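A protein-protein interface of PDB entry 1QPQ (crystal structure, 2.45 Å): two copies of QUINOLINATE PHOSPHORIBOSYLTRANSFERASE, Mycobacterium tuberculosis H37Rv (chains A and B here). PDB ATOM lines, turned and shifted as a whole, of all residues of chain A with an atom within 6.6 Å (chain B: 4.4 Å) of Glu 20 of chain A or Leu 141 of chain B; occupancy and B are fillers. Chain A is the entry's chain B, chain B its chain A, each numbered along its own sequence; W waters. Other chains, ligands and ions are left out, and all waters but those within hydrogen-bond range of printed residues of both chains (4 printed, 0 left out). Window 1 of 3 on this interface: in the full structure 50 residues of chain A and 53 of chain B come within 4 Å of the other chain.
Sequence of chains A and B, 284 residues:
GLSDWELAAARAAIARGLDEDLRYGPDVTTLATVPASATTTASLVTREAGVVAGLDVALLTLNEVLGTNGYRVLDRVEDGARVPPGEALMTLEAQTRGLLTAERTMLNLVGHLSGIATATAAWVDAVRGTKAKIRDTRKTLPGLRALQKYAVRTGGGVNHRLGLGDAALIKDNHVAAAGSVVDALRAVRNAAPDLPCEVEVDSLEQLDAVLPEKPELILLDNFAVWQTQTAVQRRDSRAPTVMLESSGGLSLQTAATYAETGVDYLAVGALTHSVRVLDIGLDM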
ATOM      1  N   ALA A  13     -28.248 -30.497  -5.706  1.00  0.00           N
ATOM      2  CA  ALA A  13     -27.730 -29.204  -5.235  1.00  0.00           C
ATOM      3  C   ALA A  13     -27.239 -28.348  -6.425  1.00  0.00           C
ATOM      4  O   ALA A  13     -27.645 -27.191  -6.540  1.00  0.00           O
ATOM      5  CB  ALA A  13     -26.597 -29.397  -4.211  1.00  0.00           C
ATOM      6  N   ALA A  15     -28.199 -28.563  -9.414  1.00  0.00           N
ATOM      7  CA  ALA A  15     -29.398 -28.229 -10.184  1.00  0.00           C
ATOM      8  C   ALA A  15     -30.154 -27.043  -9.565  1.00  0.00           C
ATOM      9  O   ALA A  15     -30.636 -26.165 -10.287  1.00  0.00           O
ATOM     10  CB  ALA A  15     -30.303 -29.422 -10.271  1.00  0.00           C
ATOM     11  N   ARG A  16     -30.287 -27.031  -8.237  1.00  0.00           N
ATOM     12  CA  ARG A  16     -30.954 -25.937  -7.546  1.00  0.00           C
ATOM     13  C   ARG A  16     -30.075 -24.673  -7.648  1.00  0.00           C
ATOM     14  O   ARG A  16     -30.572 -23.548  -7.824  1.00  0.00           O
ATOM     15  CB  ARG A  16     -31.167 -26.313  -6.092  1.00  0.00           C
ATOM     16  CG  ARG A  16     -32.037 -27.522  -5.893  1.00  0.00           C
ATOM     17  CD  ARG A  16     -32.383 -27.687  -4.447  1.00  0.00           C
ATOM     18  NE  ARG A  16     -31.331 -28.347  -3.693  1.00  0.00           N
ATOM     19  CZ  ARG A  16     -31.356 -29.638  -3.390  1.00  0.00           C
ATOM     20  NH1 ARG A  16     -32.392 -30.377  -3.778  1.00  0.00           N
ATOM     21  NH2 ARG A  16     -30.327 -30.201  -2.763  1.00  0.00           N
ATOM     22  N   GLY A  17     -28.757 -24.848  -7.579  1.00  0.00           N
ATOM     23  CA  GLY A  17     -27.886 -23.694  -7.686  1.00  0.00           C
ATOM     24  C   GLY A  17     -28.048 -22.982  -9.026  1.00  0.00           C
ATOM     25  O   GLY A  17     -28.300 -21.776  -9.069  1.00  0.00           O
ATOM     26  N   LEU A  18     -27.915 -23.740 -10.115  1.00  0.00           N
ATOM     27  CA  LEU A  18     -28.030 -23.212 -11.471  1.00  0.00           C
ATOM     28  C   LEU A  18     -29.377 -22.591 -11.704  1.00  0.00           C
ATOM     29  O   LEU A  18     -29.480 -21.545 -12.343  1.00  0.00           O
ATOM     30  CB  LEU A  18     -27.824 -24.319 -12.481  1.00  0.00           C
ATOM     31  CG  LEU A  18     -26.407 -24.812 -12.553  1.00  0.00           C
ATOM     32  CD1 LEU A  18     -26.337 -25.946 -13.468  1.00  0.00           C
ATOM     33  CD2 LEU A  18     -25.540 -23.698 -13.060  1.00  0.00           C
ATOM     34  N   ASP A  19     -30.419 -23.215 -11.172  1.00  0.00           N
ATOM     35  CA  ASP A  19     -31.746 -22.663 -11.360  1.00  0.00           C
ATOM     36  C   ASP A  19     -31.882 -21.323 -10.658  1.00  0.00           C
ATOM     37  O   ASP A  19     -32.628 -20.483 -11.106  1.00  0.00           O
ATOM     38  CB  ASP A  19     -32.849 -23.652 -10.965  1.00  0.00           C
ATOM     39  CG  ASP A  19     -34.261 -23.025 -11.025  1.00  0.00           C
ATOM     40  OD1 ASP A  19     -34.717 -22.583 -12.126  1.00  0.00           O
ATOM     41  OD2 ASP A  19     -34.922 -22.988  -9.950  1.00  0.00           O
ATOM     42  N   GLU A  20     -31.172 -21.107  -9.562  1.00  0.00           N
ATOM     43  CA  GLU A  20     -31.260 -19.816  -8.886  1.00  0.00           C
ATOM     44  C   GLU A  20     -30.599 -18.735  -9.750  1.00  0.00           C
ATOM     45  O   GLU A  20     -31.052 -17.579  -9.807  1.00  0.00           O
ATOM     46  CB  GLU A  20     -30.569 -19.900  -7.541  1.00  0.00           C
ATOM     47  CG  GLU A  20     -31.294 -20.809  -6.588  1.00  0.00           C
ATOM     48  CD  GLU A  20     -30.562 -21.002  -5.260  1.00  0.00           C
ATOM     49  OE1 GLU A  20     -29.328 -21.234  -5.267  1.00  0.00           O
ATOM     50  OE2 GLU A  20     -31.252 -20.949  -4.216  1.00  0.00           O
ATOM     51  N   ASP A  21     -29.515 -19.124 -10.409  1.00  0.00           N
ATOM     52  CA  ASP A  21     -28.774 -18.235 -11.301  1.00  0.00           C
ATOM     53  C   ASP A  21     -29.474 -17.886 -12.616  1.00  0.00           C
ATOM     54  O   ASP A  21     -29.394 -16.752 -13.083  1.00  0.00           O
ATOM     55  CB  ASP A  21     -27.422 -18.853 -11.642  1.00  0.00           C
ATOM     56  CG  ASP A  21     -26.285 -18.234 -10.858  1.00  0.00           C
ATOM     57  OD1 ASP A  21     -26.500 -17.290 -10.073  1.00  0.00           O
ATOM     58  OD2 ASP A  21     -25.149 -18.684 -11.045  1.00  0.00           O
ATOM     59  N   LEU A  22     -30.146 -18.870 -13.207  1.00  0.00           N
ATOM     60  CA  LEU A  22     -30.806 -18.709 -14.490  1.00  0.00           C
ATOM     61  C   LEU A  22     -32.281 -18.383 -14.468  1.00  0.00           C
ATOM     62  O   LEU A  22     -32.840 -18.038 -15.488  1.00  0.00           O
ATOM     63  CB  LEU A  22     -30.555 -19.951 -15.332  1.00  0.00           C
ATOM     64  CG  LEU A  22     -29.058 -20.220 -15.506  1.00  0.00           C
ATOM     65  CD1 LEU A  22     -28.766 -21.594 -16.064  1.00  0.00           C
ATOM     66  CD2 LEU A  22     -28.505 -19.166 -16.374  1.00  0.00           C
ATOM     67  N   ARG A  23     -32.883 -18.410 -13.297  1.00  0.00           N
ATOM     68  CA  ARG A  23     -34.296 -18.127 -13.121  1.00  0.00           C
ATOM     69  C   ARG A  23     -34.793 -16.809 -13.714  1.00  0.00           C
ATOM     70  O   ARG A  23     -35.971 -16.697 -14.084  1.00  0.00           O
ATOM     71  CB  ARG A  23     -34.625 -18.121 -11.625  1.00  0.00           C
ATOM     72  CG  ARG A  23     -36.008 -17.617 -11.302  1.00  0.00           C
ATOM     73  CD  ARG A  23     -36.202 -17.478  -9.834  1.00  0.00           C
ATOM     74  NE  ARG A  23     -35.610 -18.612  -9.143  1.00  0.00           N
ATOM     75  CZ  ARG A  23     -36.049 -19.869  -9.226  1.00  0.00           C
ATOM     76  NH1 ARG A  23     -37.103 -20.171  -9.986  1.00  0.00           N
ATOM     77  NH2 ARG A  23     -35.438 -20.825  -8.523  1.00  0.00           N
ATOM     78  N   TYR A  24     -33.941 -15.788 -13.767  1.00  0.00           N
ATOM     79  CA  TYR A  24     -34.391 -14.487 -14.277  1.00  0.00           C
ATOM     80  C   TYR A  24     -34.064 -14.236 -15.731  1.00  0.00           C
ATOM     81  O   TYR A  24     -34.306 -13.163 -16.253  1.00  0.00           O
ATOM     82  CB  TYR A  24     -33.832 -13.371 -13.409  1.00  0.00           C
ATOM     83  CG  TYR A  24     -34.047 -13.673 -11.980  1.00  0.00           C
ATOM     84  CD1 TYR A  24     -33.135 -14.449 -11.277  1.00  0.00           C
ATOM     85  CD2 TYR A  24     -35.234 -13.302 -11.359  1.00  0.00           C
ATOM     86  CE1 TYR A  24     -33.407 -14.864  -9.998  1.00  0.00           C
ATOM     87  CE2 TYR A  24     -35.514 -13.703 -10.083  1.00  0.00           C
ATOM     88  CZ  TYR A  24     -34.601 -14.490  -9.403  1.00  0.00           C
ATOM     89  OH  TYR A  24     -34.909 -14.895  -8.128  1.00  0.00           O
ATOM     90  N   THR A 105     -21.800 -21.110  -8.978  1.00  0.00           N
ATOM     91  CA  THR A 105     -22.386 -22.325  -8.374  1.00  0.00           C
ATOM     92  C   THR A 105     -21.308 -23.321  -7.963  1.00  0.00           C
ATOM     93  O   THR A 105     -21.334 -23.882  -6.882  1.00  0.00           O
ATOM     94  CB  THR A 105     -23.366 -23.027  -9.374  1.00  0.00           C
ATOM     95  OG1 THR A 105     -24.513 -22.192  -9.606  1.00  0.00           O
ATOM     96  CG2 THR A 105     -23.821 -24.385  -8.850  1.00  0.00           C
ATOM     97  N   ASN A 108     -19.105 -21.789  -5.068  1.00  0.00           N
ATOM     98  CA  ASN A 108     -19.895 -21.801  -3.828  1.00  0.00           C
ATOM     99  C   ASN A 108     -19.945 -23.199  -3.150  1.00  0.00           C
ATOM    100  O   ASN A 108     -19.888 -23.295  -1.918  1.00  0.00           O
ATOM    101  CB  ASN A 108     -21.331 -21.303  -4.070  1.00  0.00           C
ATOM    102  CG  ASN A 108     -21.400 -19.830  -4.357  1.00  0.00           C
ATOM    103  OD1 ASN A 108     -20.437 -19.116  -4.153  1.00  0.00           O
ATOM    104  ND2 ASN A 108     -22.543 -19.365  -4.854  1.00  0.00           N
ATOM    105  N   LEU A 109     -20.096 -24.266  -3.936  1.00  0.00           N
ATOM    106  CA  LEU A 109     -20.134 -25.601  -3.371  1.00  0.00           C
ATOM    107  C   LEU A 109     -18.771 -26.066  -2.833  1.00  0.00           C
ATOM    108  O   LEU A 109     -18.683 -26.556  -1.707  1.00  0.00           O
ATOM    109  CB  LEU A 109     -20.606 -26.611  -4.408  1.00  0.00           C
ATOM    110  CG  LEU A 109     -21.994 -27.244  -4.244  1.00  0.00           C
ATOM    111  CD1 LEU A 109     -22.355 -27.499  -2.782  1.00  0.00           C
ATOM    112  CD2 LEU A 109     -23.012 -26.338  -4.853  1.00  0.00           C
ATOM    113  N   HIS A 112     -17.614 -24.081   0.146  1.00  0.00           N
ATOM    114  CA  HIS A 112     -18.344 -24.450   1.356  1.00  0.00           C
ATOM    115  C   HIS A 112     -17.794 -25.745   1.904  1.00  0.00           C
ATOM    116  O   HIS A 112     -17.383 -25.808   3.067  1.00  0.00           O
ATOM    117  CB  HIS A 112     -19.848 -24.598   1.105  1.00  0.00           C
ATOM    118  CG  HIS A 112     -20.647 -24.925   2.338  1.00  0.00           C
ATOM    119  ND1 HIS A 112     -21.004 -23.977   3.279  1.00  0.00           N
ATOM    120  CD2 HIS A 112     -21.161 -26.095   2.783  1.00  0.00           C
ATOM    121  CE1 HIS A 112     -21.701 -24.545   4.248  1.00  0.00           C
ATOM    122  NE2 HIS A 112     -21.810 -25.833   3.970  1.00  0.00           N
ATOM    123  N   LEU A 141     -27.439 -28.040   6.919  1.00  0.00           N
ATOM    124  CA  LEU A 141     -28.337 -27.136   6.207  1.00  0.00           C
ATOM    125  C   LEU A 141     -29.278 -27.986   5.374  1.00  0.00           C
ATOM    126  O   LEU A 141     -28.835 -28.912   4.710  1.00  0.00           O
ATOM    127  CB  LEU A 141     -27.538 -26.193   5.329  1.00  0.00           C
ATOM    128  CG  LEU A 141     -27.140 -24.817   5.869  1.00  0.00           C
ATOM    129  CD1 LEU A 141     -28.027 -24.433   7.024  1.00  0.00           C
ATOM    130  CD2 LEU A 141     -25.692 -24.777   6.268  1.00  0.00           C
ATOM    131  N   LEU A 144     -28.382 -30.054   2.201  1.00  0.00           N
ATOM    132  CA  LEU A 144     -26.962 -30.274   2.047  1.00  0.00           C
ATOM    133  C   LEU A 144     -26.347 -31.282   2.992  1.00  0.00           C
ATOM    134  O   LEU A 144     -25.111 -31.471   2.987  1.00  0.00           O
ATOM    135  CB  LEU A 144     -26.218 -28.936   2.135  1.00  0.00           C
ATOM    136  CG  LEU A 144     -26.524 -27.882   1.056  1.00  0.00           C
ATOM    137  CD1 LEU A 144     -25.889 -26.577   1.450  1.00  0.00           C
ATOM    138  CD2 LEU A 144     -25.991 -28.314  -0.290  1.00  0.00           C
ATOM    139  N   THR B 140     -24.008 -17.369  -2.240  1.00  0.00           N
ATOM    140  CA  THR B 140     -25.039 -18.005  -1.439  1.00  0.00           C
ATOM    141  C   THR B 140     -24.956 -19.522  -1.559  1.00  0.00           C
ATOM    142  O   THR B 140     -24.212 -20.030  -2.382  1.00  0.00           O
ATOM    143  CB  THR B 140     -26.392 -17.482  -1.886  1.00  0.00           C
ATOM    144  OG1 THR B 140     -26.531 -17.653  -3.309  1.00  0.00           O
ATOM    145  CG2 THR B 140     -26.465 -15.998  -1.563  1.00  0.00           C
ATOM    146  N   LEU B 141     -25.660 -20.259  -0.709  1.00  0.00           N
ATOM    147  CA  LEU B 141     -25.603 -21.722  -0.761  1.00  0.00           C
ATOM    148  C   LEU B 141     -26.692 -22.189  -1.692  1.00  0.00           C
ATOM    149  O   LEU B 141     -27.802 -21.646  -1.689  1.00  0.00           O
ATOM    150  CB  LEU B 141     -25.809 -22.364   0.619  1.00  0.00           C
ATOM    151  CG  LEU B 141     -24.625 -22.636   1.562  1.00  0.00           C
ATOM    152  CD1 LEU B 141     -23.370 -22.852   0.753  1.00  0.00           C
ATOM    153  CD2 LEU B 141     -24.426 -21.510   2.552  1.00  0.00           C
ATOM    154  N   PRO B 142     -26.405 -23.228  -2.471  1.00  0.00           N
ATOM    155  CA  PRO B 142     -27.361 -23.783  -3.425  1.00  0.00           C
ATOM    156  C   PRO B 142     -28.666 -24.227  -2.792  1.00  0.00           C
ATOM    157  O   PRO B 142     -28.700 -25.079  -1.919  1.00  0.00           O
ATOM    158  CB  PRO B 142     -26.596 -24.950  -4.053  1.00  0.00           C
ATOM    159  CG  PRO B 142     -25.572 -25.281  -3.032  1.00  0.00           C
ATOM    160  CD  PRO B 142     -25.133 -23.956  -2.510  1.00  0.00           C
ATOM    161  N   GLY B 143     -29.748 -23.610  -3.238  1.00  0.00           N
ATOM    162  CA  GLY B 143     -31.043 -23.955  -2.719  1.00  0.00           C
ATOM    163  C   GLY B 143     -31.478 -23.030  -1.624  1.00  0.00           C
ATOM    164  O   GLY B 143     -32.625 -23.085  -1.219  1.00  0.00           O
ATOM    165  N   LEU B 144     -30.580 -22.181  -1.130  1.00  0.00           N
ATOM    166  CA  LEU B 144     -30.962 -21.266  -0.067  1.00  0.00           C
ATOM    167  C   LEU B 144     -30.878 -19.773  -0.365  1.00  0.00           C
ATOM    168  O   LEU B 144     -31.121 -18.963   0.530  1.00  0.00           O
ATOM    169  CB  LEU B 144     -30.180 -21.577   1.205  1.00  0.00           C
ATOM    170  CG  LEU B 144     -30.400 -22.955   1.828  1.00  0.00           C
ATOM    171  CD1 LEU B 144     -29.336 -23.189   2.851  1.00  0.00           C
ATOM    172  CD2 LEU B 144     -31.769 -23.070   2.465  1.00  0.00           C
ATOM    173  N   ARG B 145     -30.604 -19.386  -1.607  1.00  0.00           N
ATOM    174  CA  ARG B 145     -30.483 -17.969  -1.933  1.00  0.00           C
ATOM    175  C   ARG B 145     -31.641 -17.070  -1.534  1.00  0.00           C
ATOM    176  O   ARG B 145     -31.423 -15.990  -0.974  1.00  0.00           O
ATOM    177  CB  ARG B 145     -30.163 -17.768  -3.419  1.00  0.00           C
ATOM    178  CG  ARG B 145     -30.190 -16.306  -3.844  1.00  0.00           C
ATOM    179  CD  ARG B 145     -29.569 -16.103  -5.201  1.00  0.00           C
ATOM    180  NE  ARG B 145     -28.232 -16.664  -5.310  1.00  0.00           N
ATOM    181  CZ  ARG B 145     -27.613 -16.888  -6.480  1.00  0.00           C
ATOM    182  NH1 ARG B 145     -28.214 -16.583  -7.625  1.00  0.00           N
ATOM    183  NH2 ARG B 145     -26.422 -17.499  -6.526  1.00  0.00           N
ATOM    184  N   GLN B 148     -31.581 -16.681   2.304  1.00  0.00           N
ATOM    185  CA  GLN B 148     -30.406 -15.897   2.706  1.00  0.00           C
ATOM    186  C   GLN B 148     -30.556 -14.435   2.315  1.00  0.00           C
ATOM    187  O   GLN B 148     -30.211 -13.558   3.117  1.00  0.00           O
ATOM    188  CB  GLN B 148     -29.116 -16.470   2.136  1.00  0.00           C
ATOM    189  CG  GLN B 148     -28.875 -17.803   2.701  1.00  0.00           C
ATOM    190  CD  GLN B 148     -27.577 -18.369   2.288  1.00  0.00           C
ATOM    191  OE1 GLN B 148     -26.871 -18.978   3.071  1.00  0.00           O
ATOM    192  NE2 GLN B 148     -27.266 -18.225   1.045  1.00  0.00           N
ATOM    193  N   LEU B 162     -30.343 -11.080  -7.824  1.00  0.00           N
ATOM    194  CA  LEU B 162     -30.721 -12.432  -7.438  1.00  0.00           C
ATOM    195  C   LEU B 162     -30.146 -13.526  -8.338  1.00  0.00           C
ATOM    196  O   LEU B 162     -30.056 -14.688  -7.937  1.00  0.00           O
ATOM    197  CB  LEU B 162     -32.242 -12.546  -7.366  1.00  0.00           C
ATOM    198  CG  LEU B 162     -32.879 -11.557  -6.383  1.00  0.00           C
ATOM    199  CD1 LEU B 162     -34.371 -11.546  -6.576  1.00  0.00           C
ATOM    200  CD2 LEU B 162     -32.507 -11.933  -4.954  1.00  0.00           C
ATOM    201  N   GLY B 163     -29.736 -13.160  -9.540  1.00  0.00           N
ATOM    202  CA  GLY B 163     -29.186 -14.144 -10.431  1.00  0.00           C
ATOM    203  C   GLY B 163     -28.403 -13.456 -11.509  1.00  0.00           C
ATOM    204  O   GLY B 163     -28.153 -12.255 -11.431  1.00  0.00           O
ATOM    205  N   THR B 272     -23.392 -14.219   3.594  1.00  0.00           N
ATOM    206  CA  THR B 272     -24.068 -15.454   3.180  1.00  0.00           C
ATOM    207  C   THR B 272     -23.171 -16.686   3.062  1.00  0.00           C
ATOM    208  O   THR B 272     -23.664 -17.823   3.093  1.00  0.00           O
ATOM    209  CB  THR B 272     -24.884 -15.215   1.888  1.00  0.00           C
ATOM    210  OG1 THR B 272     -24.027 -14.713   0.836  1.00  0.00           O
ATOM    211  CG2 THR B 272     -25.911 -14.172   2.156  1.00  0.00           C
HETATM  212  O   HOH W   1     -29.425 -27.694  -1.846  1.00  0.00           O
HETATM  213  O   HOH W   2     -32.801 -16.488  -7.843  1.00  0.00           O
HETATM  214  O   HOH W   3     -25.174 -20.766  -5.293  1.00  0.00           O
HETATM  215  O   HOH W   4     -27.258 -19.943  -3.847  1.00  0.00           O
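O of Leu 162 of chain B lies within hydrogen-bond range of NH1 of Arg 145 of chain B.
The side-chain hydroxyl (OG1) of Thr 140 of chain B sits at hydrogen-bond distance from the guanidinium group (NE) of Arg 145 of chain B.
The backbone NH of Leu 141 of chain B lies close to the side-chain amide nitrogen of Gln 148 of chain B, at 3.1 Å.
Hydrophobic or aromatic side chains of chain A within 4 Å of the printed part of chain B: Tyr 24, Leu 109 and His 112.
Among the printed residues, Asp or Glu carboxylates within 4 Å of a Lys or Arg side-chain nitrogen of the other chain: Asp 21 of chain A with Arg 145 of chain B (3.1 Å).
Water W4 lies within hydrogen-bond range of OG1 of Thr 140 of chain B, O of Leu 141 of chain B and OE1 of Glu 20 of chain A.
Water W2 lies within hydrogen-bond range of the side-chain hydroxyl of Tyr 24 of chain A, the backbone carbonyl oxygen of Glu 20 of chain A and the backbone carbonyl oxygen of Leu 162 of chain B.
Water W1 lies within hydrogen-bond range of the backbone carbonyl oxygen (O) of Pro 142 of chain B and the guanidinium group (NE) of Arg 16 of chain A.
Water W3 bridges ND2 of Asn 108 of chain A and O of Thr 140 of chain B.
Glu 20 of chain A touches just these residues of chain B: Leu 141 (3.9 Å), Pro 142 (3.7 Å), Gly 143 (3.2 Å), Leu 144 (3.4 Å), Arg 145 (3.1 Å), Leu 162 (3.6 Å) and Gly 163 (3.96 Å).
Of chain A, only Glu 20 and His 112 come within 4 Å of Leu 141 of chain B.
Of the printed residues of chain B, Asp 21 of chain A touches Arg 145 (3.1 Å) and Gly 163 (3.7 Å).
Printed residues of chain A within 4 Å of Pro 142 of chain B: Ala 13, Glu 20 and Leu 109.
Of the printed residues of chain B, Leu 109 of chain A touches Pro 142.
Printed residues of chain B within 4 Å of His 112 of chain A: Leu 141.
Of the printed residues of chain B, Tyr 24 of chain A touches Leu 162.
Leu 144 of chain A touches none of the printed residues of chain B.
Gly 17 of chain A touches none of the printed residues of chain B.
2 positions are printed for both chains.
Of the 14 pairs that touch across the chains among the printed residues, none has its exchanged pair printed and touching as well.
CB of Pro 142 of chain B touches O of Ala 13 of chain A, 3.5 Å away.
OE1 of Glu 20 of chain A touches O of Leu 141 of chain B, 3.9 Å away.
Glu 20 of chain A touches Pro 142 of chain B.
O of Glu 20 of chain A touches O of Leu 162 of chain B (3.6 Å).
Glu 20 of chain A touches Gly 163 of chain B (O to CA, 3.96 Å).
Asp 21 of chain A touches Gly 163 of chain B (O to CA, 3.7 Å).
Leu 162 of chain B touches Tyr 24 of chain A.
CD2 of Leu 109 of chain A touches CG of Pro 142 of chain B (3.3 Å).
Leu 141 of chain B touches His 112 of chain A.
The side-chain carboxylate (OE2) of Glu 20 of chain A sits at hydrogen-bond distance from the backbone NH (N) of Leu 144 of chain B, 3.4 Å away.
The backbone carbonyl oxygen (O) of Thr 140 of chain B lies within hydrogen-bond range of the side-chain amide nitrogen (ND2) of Asn 108 of chain A (3.1 Å).
The side-chain carboxylate (OD1) of Asp 21 of chain A lies within salt-bridge range of the guanidinium group (NH1) of Arg 145 of chain B (3.1 Å).
OE1 of Glu 20 of chain A sits at hydrogen-bond distance from N of Gly 143 of chain B, at 3.2 Å.
The side-chain carboxylate (OE2) of Glu 20 of chain A lies within hydrogen-bond range of the backbone NH (N) of Arg 145 of chain B, at 3.1 Å.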
